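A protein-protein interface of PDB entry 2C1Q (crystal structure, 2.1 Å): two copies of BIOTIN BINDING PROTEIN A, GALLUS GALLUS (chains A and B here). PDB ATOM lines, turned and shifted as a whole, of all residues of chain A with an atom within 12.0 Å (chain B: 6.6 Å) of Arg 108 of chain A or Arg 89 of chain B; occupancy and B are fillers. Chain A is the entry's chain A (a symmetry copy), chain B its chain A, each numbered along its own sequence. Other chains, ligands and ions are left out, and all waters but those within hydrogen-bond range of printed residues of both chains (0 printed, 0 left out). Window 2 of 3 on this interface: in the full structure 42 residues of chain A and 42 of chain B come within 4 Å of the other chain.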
ATOM      1  N   ARG A 102      -3.603  -6.473   4.985  1.00  0.00           N
ATOM      2  CA  ARG A 102      -2.139  -6.374   4.945  1.00  0.00           C
ATOM      3  C   ARG A 102      -1.745  -5.139   4.169  1.00  0.00           C
ATOM      4  O   ARG A 102      -2.006  -5.066   2.972  1.00  0.00           O
ATOM      5  CB  ARG A 102      -1.548  -7.579   4.226  1.00  0.00           C
ATOM      6  CG  ARG A 102       0.004  -7.568   4.078  1.00  0.00           C
ATOM      7  CD  ARG A 102       0.491  -8.190   5.278  1.00  0.00           C
ATOM      8  NE  ARG A 102       1.925  -8.376   5.413  1.00  0.00           N
ATOM      9  CZ  ARG A 102       2.398  -9.367   6.155  1.00  0.00           C
ATOM     10  NH1 ARG A 102       1.530 -10.230   6.713  1.00  0.00           N
ATOM     11  NH2 ARG A 102       3.686  -9.520   6.325  1.00  0.00           N
ATOM     12  N   GLU A 103      -1.138  -4.168   4.848  1.00  0.00           N
ATOM     13  CA  GLU A 103      -0.586  -3.010   4.163  1.00  0.00           C
ATOM     14  C   GLU A 103       0.818  -3.282   3.629  1.00  0.00           C
ATOM     15  O   GLU A 103       1.607  -4.003   4.233  1.00  0.00           O
ATOM     16  CB  GLU A 103      -0.669  -1.731   5.031  1.00  0.00           C
ATOM     17  CG  GLU A 103      -2.128  -1.472   5.540  1.00  0.00           C
ATOM     18  CD  GLU A 103      -2.703  -0.096   5.204  1.00  0.00           C
ATOM     19  OE1 GLU A 103      -2.247   0.893   5.834  1.00  0.00           O
ATOM     20  OE2 GLU A 103      -3.633   0.008   4.345  1.00  0.00           O
ATOM     21  N   GLU A 104       1.115  -2.713   2.462  1.00  0.00           N
ATOM     22  CA  GLU A 104       2.449  -2.832   1.888  1.00  0.00           C
ATOM     23  C   GLU A 104       3.419  -1.983   2.700  1.00  0.00           C
ATOM     24  O   GLU A 104       3.135  -0.818   2.979  1.00  0.00           O
ATOM     25  CB  GLU A 104       2.437  -2.413   0.417  1.00  0.00           C
ATOM     26  CG  GLU A 104       3.750  -2.677  -0.330  1.00  0.00           C
ATOM     27  CD  GLU A 104       3.773  -2.035  -1.727  1.00  0.00           C
ATOM     28  OE1 GLU A 104       3.144  -0.952  -1.942  1.00  0.00           O
ATOM     29  OE2 GLU A 104       4.416  -2.617  -2.619  1.00  0.00           O
ATOM     30  N   VAL A 105       4.554  -2.566   3.091  1.00  0.00           N
ATOM     31  CA  VAL A 105       5.533  -1.800   3.859  1.00  0.00           C
ATOM     32  C   VAL A 105       6.893  -1.651   3.144  1.00  0.00           C
ATOM     33  O   VAL A 105       7.288  -2.533   2.382  1.00  0.00           O
ATOM     34  CB  VAL A 105       5.690  -2.300   5.339  1.00  0.00           C
ATOM     35  CG1 VAL A 105       4.393  -2.122   6.111  1.00  0.00           C
ATOM     36  CG2 VAL A 105       6.197  -3.713   5.385  1.00  0.00           C
ATOM     37  N   PRO A 106       7.605  -0.533   3.388  1.00  0.00           N
ATOM     38  CA  PRO A 106       8.877  -0.284   2.690  1.00  0.00           C
ATOM     39  C   PRO A 106       9.983  -1.316   2.976  1.00  0.00           C
ATOM     40  O   PRO A 106      10.701  -1.703   2.051  1.00  0.00           O
ATOM     41  CB  PRO A 106       9.285   1.110   3.175  1.00  0.00           C
ATOM     42  CG  PRO A 106       8.590   1.304   4.428  1.00  0.00           C
ATOM     43  CD  PRO A 106       7.271   0.578   4.289  1.00  0.00           C
ATOM     44  N   SER A 107      10.137  -1.769   4.213  1.00  0.00           N
ATOM     45  CA  SER A 107      11.186  -2.769   4.465  1.00  0.00           C
ATOM     46  C   SER A 107      10.732  -3.893   5.366  1.00  0.00           C
ATOM     47  O   SER A 107       9.684  -3.788   6.003  1.00  0.00           O
ATOM     48  CB  SER A 107      12.496  -2.114   4.950  1.00  0.00           C
ATOM     49  OG  SER A 107      12.512  -1.853   6.342  1.00  0.00           O
ATOM     50  N   ARG A 108      11.517  -4.968   5.400  1.00  0.00           N
ATOM     51  CA  ARG A 108      11.162  -6.163   6.150  1.00  0.00           C
ATOM     52  C   ARG A 108      10.911  -5.886   7.637  1.00  0.00           C
ATOM     53  O   ARG A 108      10.099  -6.569   8.289  1.00  0.00           O
ATOM     54  CB  ARG A 108      12.216  -7.266   5.966  1.00  0.00           C
ATOM     55  CG  ARG A 108      11.686  -8.638   6.345  1.00  0.00           C
ATOM     56  CD  ARG A 108      12.737  -9.733   6.367  1.00  0.00           C
ATOM     57  NE  ARG A 108      14.051  -9.241   6.804  1.00  0.00           N
ATOM     58  CZ  ARG A 108      14.944  -9.950   7.499  1.00  0.00           C
ATOM     59  NH1 ARG A 108      14.683 -11.203   7.870  1.00  0.00           N
ATOM     60  NH2 ARG A 108      16.114  -9.396   7.829  1.00  0.00           N
ATOM     61  N   LYS A 109      11.595  -4.870   8.153  1.00  0.00           N
ATOM     62  CA  LYS A 109      11.554  -4.522   9.570  1.00  0.00           C
ATOM     63  C   LYS A 109      10.223  -3.887   9.962  1.00  0.00           C
ATOM     64  O   LYS A 109       9.898  -3.842  11.137  1.00  0.00           O
ATOM     65  CB  LYS A 109      12.700  -3.558   9.918  1.00  0.00           C
ATOM     66  CG  LYS A 109      12.355  -2.085   9.600  1.00  0.00           C
ATOM     67  CD  LYS A 109      13.548  -1.163   9.641  1.00  0.00           C
ATOM     68  CE  LYS A 109      13.114   0.245   9.236  1.00  0.00           C
ATOM     69  NZ  LYS A 109      14.300   1.092   8.909  1.00  0.00           N
ATOM     70  N   ASP A 110       9.470  -3.379   8.994  1.00  0.00           N
ATOM     71  CA  ASP A 110       8.142  -2.830   9.276  1.00  0.00           C
ATOM     72  C   ASP A 110       7.040  -3.894   9.192  1.00  0.00           C
ATOM     73  O   ASP A 110       5.888  -3.563   9.356  1.00  0.00           O
ATOM     74  CB  ASP A 110       7.766  -1.722   8.284  1.00  0.00           C
ATOM     75  CG  ASP A 110       8.680  -0.541   8.336  1.00  0.00           C
ATOM     76  OD1 ASP A 110       9.079  -0.091   9.435  1.00  0.00           O
ATOM     77  OD2 ASP A 110       8.975  -0.023   7.245  1.00  0.00           O
ATOM     78  N   THR A 111       7.376  -5.144   8.878  1.00  0.00           N
ATOM     79  CA  THR A 111       6.327  -6.134   8.733  1.00  0.00           C
ATOM     80  C   THR A 111       5.527  -6.320  10.033  1.00  0.00           C
ATOM     81  O   THR A 111       4.341  -6.583   9.957  1.00  0.00           O
ATOM     82  CB  THR A 111       6.783  -7.558   8.160  1.00  0.00           C
ATOM     83  OG1 THR A 111       7.388  -8.329   9.183  1.00  0.00           O
ATOM     84  CG2 THR A 111       7.713  -7.473   7.065  1.00  0.00           C
ATOM     85  N   TRP A 112       6.144  -6.165  11.214  1.00  0.00           N
ATOM     86  CA  TRP A 112       5.422  -6.381  12.485  1.00  0.00           C
ATOM     87  C   TRP A 112       4.086  -5.613  12.562  1.00  0.00           C
ATOM     88  O   TRP A 112       3.153  -6.084  13.184  1.00  0.00           O
ATOM     89  CB  TRP A 112       6.284  -6.061  13.733  1.00  0.00           C
ATOM     90  CG  TRP A 112       6.441  -4.571  13.906  1.00  0.00           C
ATOM     91  CD1 TRP A 112       7.416  -3.772  13.349  1.00  0.00           C
ATOM     92  CD2 TRP A 112       5.575  -3.702  14.637  1.00  0.00           C
ATOM     93  NE1 TRP A 112       7.200  -2.465  13.690  1.00  0.00           N
ATOM     94  CE2 TRP A 112       6.083  -2.390  14.491  1.00  0.00           C
ATOM     95  CE3 TRP A 112       4.426  -3.909  15.433  1.00  0.00           C
ATOM     96  CZ2 TRP A 112       5.483  -1.293  15.096  1.00  0.00           C
ATOM     97  CZ3 TRP A 112       3.819  -2.805  16.015  1.00  0.00           C
ATOM     98  CH2 TRP A 112       4.348  -1.521  15.851  1.00  0.00           C
ATOM     99  N   LYS A 113       4.012  -4.434  11.956  1.00  0.00           N
ATOM    100  CA  LYS A 113       2.818  -3.576  12.037  1.00  0.00           C
ATOM    101  C   LYS A 113       1.887  -3.630  10.809  1.00  0.00           C
ATOM    102  O   LYS A 113       0.943  -2.834  10.684  1.00  0.00           O
ATOM    103  CB  LYS A 113       3.246  -2.119  12.294  1.00  0.00           C
ATOM    104  CG  LYS A 113       4.190  -1.529  11.263  1.00  0.00           C
ATOM    105  CD  LYS A 113       4.341  -0.008  11.458  1.00  0.00           C
ATOM    106  CE  LYS A 113       4.491   0.679  10.106  1.00  0.00           C
ATOM    107  NZ  LYS A 113       5.239   1.973  10.228  1.00  0.00           N
ATOM    108  N   ALA A 114       2.145  -4.565   9.909  1.00  0.00           N
ATOM    109  CA  ALA A 114       1.515  -4.568   8.599  1.00  0.00           C
ATOM    110  C   ALA A 114       0.118  -5.222   8.530  1.00  0.00           C
ATOM    111  O   ALA A 114      -0.548  -5.134   7.489  1.00  0.00           O
ATOM    112  CB  ALA A 114       2.475  -5.220   7.562  1.00  0.00           C
ATOM    113  N   THR A 115      -0.339  -5.856   9.607  1.00  0.00           N
ATOM    114  CA  THR A 115      -1.532  -6.716   9.505  1.00  0.00           C
ATOM    115  C   THR A 115      -2.547  -6.321  10.537  1.00  0.00           C
ATOM    116  O   THR A 115      -2.288  -6.416  11.711  1.00  0.00           O
ATOM    117  CB  THR A 115      -1.164  -8.208   9.724  1.00  0.00           C
ATOM    118  OG1 THR A 115      -0.132  -8.559   8.817  1.00  0.00           O
ATOM    119  CG2 THR A 115      -2.327  -9.120   9.466  1.00  0.00           C
ATOM    120  N   PHE B  86      10.185  -9.893   0.516  1.00  0.00           N
ATOM    121  CA  PHE B  86      11.313  -8.985   0.729  1.00  0.00           C
ATOM    122  C   PHE B  86      12.579  -9.641   0.248  1.00  0.00           C
ATOM    123  O   PHE B  86      12.708 -10.858   0.309  1.00  0.00           O
ATOM    124  CB  PHE B  86      11.461  -8.616   2.211  1.00  0.00           C
ATOM    125  CG  PHE B  86      10.258  -7.918   2.773  1.00  0.00           C
ATOM    126  CD1 PHE B  86      10.148  -6.537   2.705  1.00  0.00           C
ATOM    127  CD2 PHE B  86       9.210  -8.649   3.332  1.00  0.00           C
ATOM    128  CE1 PHE B  86       9.026  -5.899   3.198  1.00  0.00           C
ATOM    129  CE2 PHE B  86       8.077  -8.005   3.813  1.00  0.00           C
ATOM    130  CZ  PHE B  86       7.993  -6.644   3.755  1.00  0.00           C
ATOM    131  N   VAL B  87      13.497  -8.830  -0.262  1.00  0.00           N
ATOM    132  CA  VAL B  87      14.848  -9.290  -0.585  1.00  0.00           C
ATOM    133  C   VAL B  87      15.826  -8.546   0.305  1.00  0.00           C
ATOM    134  O   VAL B  87      15.813  -7.307   0.359  1.00  0.00           O
ATOM    135  CB  VAL B  87      15.259  -9.012  -2.050  1.00  0.00           C
ATOM    136  CG1 VAL B  87      16.408  -9.934  -2.447  1.00  0.00           C
ATOM    137  CG2 VAL B  87      14.089  -9.182  -2.985  1.00  0.00           C
ATOM    138  N   ASP B  88      16.677  -9.295   0.996  1.00  0.00           N
ATOM    139  CA  ASP B  88      17.687  -8.675   1.855  1.00  0.00           C
ATOM    140  C   ASP B  88      18.998  -8.304   1.105  1.00  0.00           C
ATOM    141  O   ASP B  88      19.018  -8.204  -0.135  1.00  0.00           O
ATOM    142  CB  ASP B  88      17.931  -9.532   3.112  1.00  0.00           C
ATOM    143  CG  ASP B  88      18.719 -10.790   2.825  1.00  0.00           C
ATOM    144  OD1 ASP B  88      19.423 -10.820   1.794  1.00  0.00           O
ATOM    145  OD2 ASP B  88      18.641 -11.743   3.638  1.00  0.00           O
ATOM    146  N   ARG B  89      20.069  -8.096   1.878  1.00  0.00           N
ATOM    147  CA  ARG B  89      21.399  -7.702   1.374  1.00  0.00           C
ATOM    148  C   ARG B  89      21.971  -8.724   0.382  1.00  0.00           C
ATOM    149  O   ARG B  89      22.168  -8.418  -0.801  1.00  0.00           O
ATOM    150  CB  ARG B  89      22.381  -7.492   2.542  1.00  0.00           C
ATOM    151  CG  ARG B  89      21.878  -6.556   3.648  1.00  0.00           C
ATOM    152  CD  ARG B  89      20.830  -7.242   4.568  1.00  0.00           C
ATOM    153  NE  ARG B  89      19.587  -6.467   4.671  1.00  0.00           N
ATOM    154  CZ  ARG B  89      18.533  -6.811   5.412  1.00  0.00           C
ATOM    155  NH1 ARG B  89      18.548  -7.923   6.139  1.00  0.00           N
ATOM    156  NH2 ARG B  89      17.456  -6.036   5.428  1.00  0.00           N
ATOM    157  N   ARG B  90      22.208  -9.941   0.871  1.00  0.00           N
ATOM    158  CA  ARG B  90      22.836 -10.999   0.084  1.00  0.00           C
ATOM    159  C   ARG B  90      21.868 -11.697  -0.900  1.00  0.00           C
ATOM    160  O   ARG B  90      22.046 -12.876  -1.246  1.00  0.00           O
ATOM    161  CB  ARG B  90      23.522 -12.012   1.021  1.00  0.00           C
ATOM    162  CG  ARG B  90      24.501 -11.380   2.030  1.00  0.00           C
ATOM    163  CD  ARG B  90      25.300 -12.453   2.775  1.00  0.00           C
ATOM    164  NE  ARG B  90      26.496 -11.912   3.439  1.00  0.00           N
ATOM    165  CZ  ARG B  90      27.467 -12.646   3.989  1.00  0.00           C
ATOM    166  NH1 ARG B  90      27.421 -13.978   3.961  1.00  0.00           N
ATOM    167  NH2 ARG B  90      28.501 -12.045   4.568  1.00  0.00           N
ATOM    168  N   GLY B  91      20.855 -10.953  -1.353  1.00  0.00           N
ATOM    169  CA  GLY B  91      19.911 -11.412  -2.384  1.00  0.00           C
ATOM    170  C   GLY B  91      18.841 -12.411  -1.962  1.00  0.00           C
ATOM    171  O   GLY B  91      18.108 -12.919  -2.812  1.00  0.00           O
ATOM    172  N   LYS B  92      18.741 -12.683  -0.660  1.00  0.00           N
ATOM    173  CA  LYS B  92      17.819 -13.692  -0.130  1.00  0.00           C
ATOM    174  C   LYS B  92      16.380 -13.156  -0.025  1.00  0.00           C
ATOM    175  O   LYS B  92      16.147 -12.090   0.560  1.00  0.00           O
ATOM    176  CB  LYS B  92      18.308 -14.180   1.229  1.00  0.00           C
ATOM    177  CG  LYS B  92      17.599 -15.403   1.785  1.00  0.00           C
ATOM    178  CD  LYS B  92      17.751 -15.440   3.307  1.00  0.00           C
ATOM    179  CE  LYS B  92      17.491 -16.837   3.884  1.00  0.00           C
ATOM    180  NZ  LYS B  92      17.643 -16.835   5.370  1.00  0.00           N
ATOM    181  N   MET B  94      12.286 -13.501   1.038  1.00  0.00           N
ATOM    182  CA  MET B  94      11.453 -14.040   2.112  1.00  0.00           C
ATOM    183  C   MET B  94      10.035 -13.558   1.976  1.00  0.00           C
ATOM    184  O   MET B  94       9.814 -12.380   1.797  1.00  0.00           O
ATOM    185  CB  MET B  94      11.973 -13.595   3.486  1.00  0.00           C
ATOM    186  CG  MET B  94      13.495 -13.686   3.658  1.00  0.00           C
ATOM    187  SD  MET B  94      13.998 -13.016   5.240  1.00  0.00           S
ATOM    188  CE  MET B  94      13.759 -14.467   6.268  1.00  0.00           C
ATOM    189  N   GLU B  96       6.848 -12.828   4.077  1.00  0.00           N
ATOM    190  CA  GLU B  96       6.271 -12.585   5.398  1.00  0.00           C
ATOM    191  C   GLU B  96       4.762 -12.680   5.275  1.00  0.00           C
ATOM    192  O   GLU B  96       4.145 -11.883   4.540  1.00  0.00           O
ATOM    193  CB  GLU B  96       6.640 -11.189   5.922  1.00  0.00           C
ATOM    194  CG  GLU B  96       8.117 -10.938   6.081  1.00  0.00           C
ATOM    195  CD  GLU B  96       8.750 -11.729   7.236  1.00  0.00           C
ATOM    196  OE1 GLU B  96       8.032 -12.211   8.171  1.00  0.00           O
ATOM    197  OE2 GLU B  96       9.984 -11.861   7.187  1.00  0.00           O
ATOM    198  N   VAL B 121       7.052 -17.600   7.779  1.00  0.00           N
ATOM    199  CA  VAL B 121       8.093 -16.971   6.955  1.00  0.00           C
ATOM    200  C   VAL B 121       8.519 -18.009   5.939  1.00  0.00           C
ATOM    201  O   VAL B 121       8.876 -19.116   6.315  1.00  0.00           O
ATOM    202  CB  VAL B 121       9.326 -16.515   7.761  1.00  0.00           C
ATOM    203  CG1 VAL B 121      10.313 -15.719   6.839  1.00  0.00           C
ATOM    204  CG2 VAL B 121       8.907 -15.616   8.896  1.00  0.00           C
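The backbone carbonyl oxygen of Glu 96 of chain B is in hydrogen-bond range of the guanidinium group of Arg 102 of chain A, 3.0 Å away. NH1 of Arg 89 of chain B lies close to NH2 of Arg 108 of chain A, 3.3 Å away. The side-chain sulfur (SD) of Met 94 of chain B lies within hydrogen-bond range of the guanidinium group (NH1) of Arg 108 of chain A, at 3.3 Å.
The backbone carbonyl oxygen of Phe 86 of chain B lies within hydrogen-bond range of the backbone NH of Met 94 of chain B (2.8 Å). O of Arg 108 of chain A sits close to OG1 of Thr 111 of chain A. The side-chain hydroxyl of Thr 115 of chain A sits at hydrogen-bond distance from the guanidinium group of Arg 102 of chain A (3.2 Å).
Among the printed residues, merely in contact across the chains: Val 105 of chain A with Phe 86 of chain B (3.8 Å), Ser 107 of chain A with Phe 86 of chain B (3.4 Å), Arg 108 of chain A with Phe 86 of chain B (3.4 Å), Arg 108 of chain A with Glu 96 of chain B (3.6 Å), Thr 111 of chain A with Phe 86 of chain B (3.3 Å) and Thr 111 of chain A with Glu 96 of chain B (3.6 Å).
Arg 108 of chain A touches just these residues of chain B: Phe 86 (3.4 Å), Arg 89 (3.3 Å), Met 94 (3.3 Å) and Glu 96 (3.6 Å). Arg 89 of chain B touches just one residue of chain A: Arg 108 (3.3 Å). Phe 86 of chain B touches just these residues of chain A: Val 105 (3.8 Å), Ser 107 (3.4 Å), Arg 108 (3.4 Å) and Thr 111 (3.3 Å). No residue of chain A comes within 4 Å of Asp 88 of chain B. No residue of chain A comes within 4 Å of Gly 91 of chain B. No residue of chain A comes within 4 Å of Lys 92 of chain B. Met 94 of chain B touches just one residue of chain A: Arg 108. Of the printed residues of chain B, Ser 107 of chain A touches Phe 86. Of the printed residues of chain B, Thr 111 of chain A touches Phe 86 (3.3 Å) and Glu 96 (3.6 Å). Of the printed residues of chain B, Arg 102 of chain A touches Glu 96. Of the printed residues of chain B, Val 105 of chain A touches Phe 86. Thr 115 of chain A touches none of the printed residues of chain B. Trp 112 of chain A touches none of the printed residues of chain B. The nearest residue of chain B that does not touch Arg 108 of chain A is Asp 88 of chain B (5.1 Å). The nearest printed residue of chain B that does not touch Ser 107 of chain A is Arg 89 of chain B (6.3 Å).
Of the 10 printed residues of chain B, 4 touch a printed residue of chain A. Hydrophobic or aromatic side chains of chain A within 4 Å of the printed part of chain B: Val 105. Among the printed residues, no Asp or Glu carboxylate lies within 4 Å of a Lys or Arg side-chain nitrogen of the other chain.
No position is printed for both chains. Of the 9 pairs that touch across the chains among the printed residues, none has its exchanged pair printed and touching as well.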
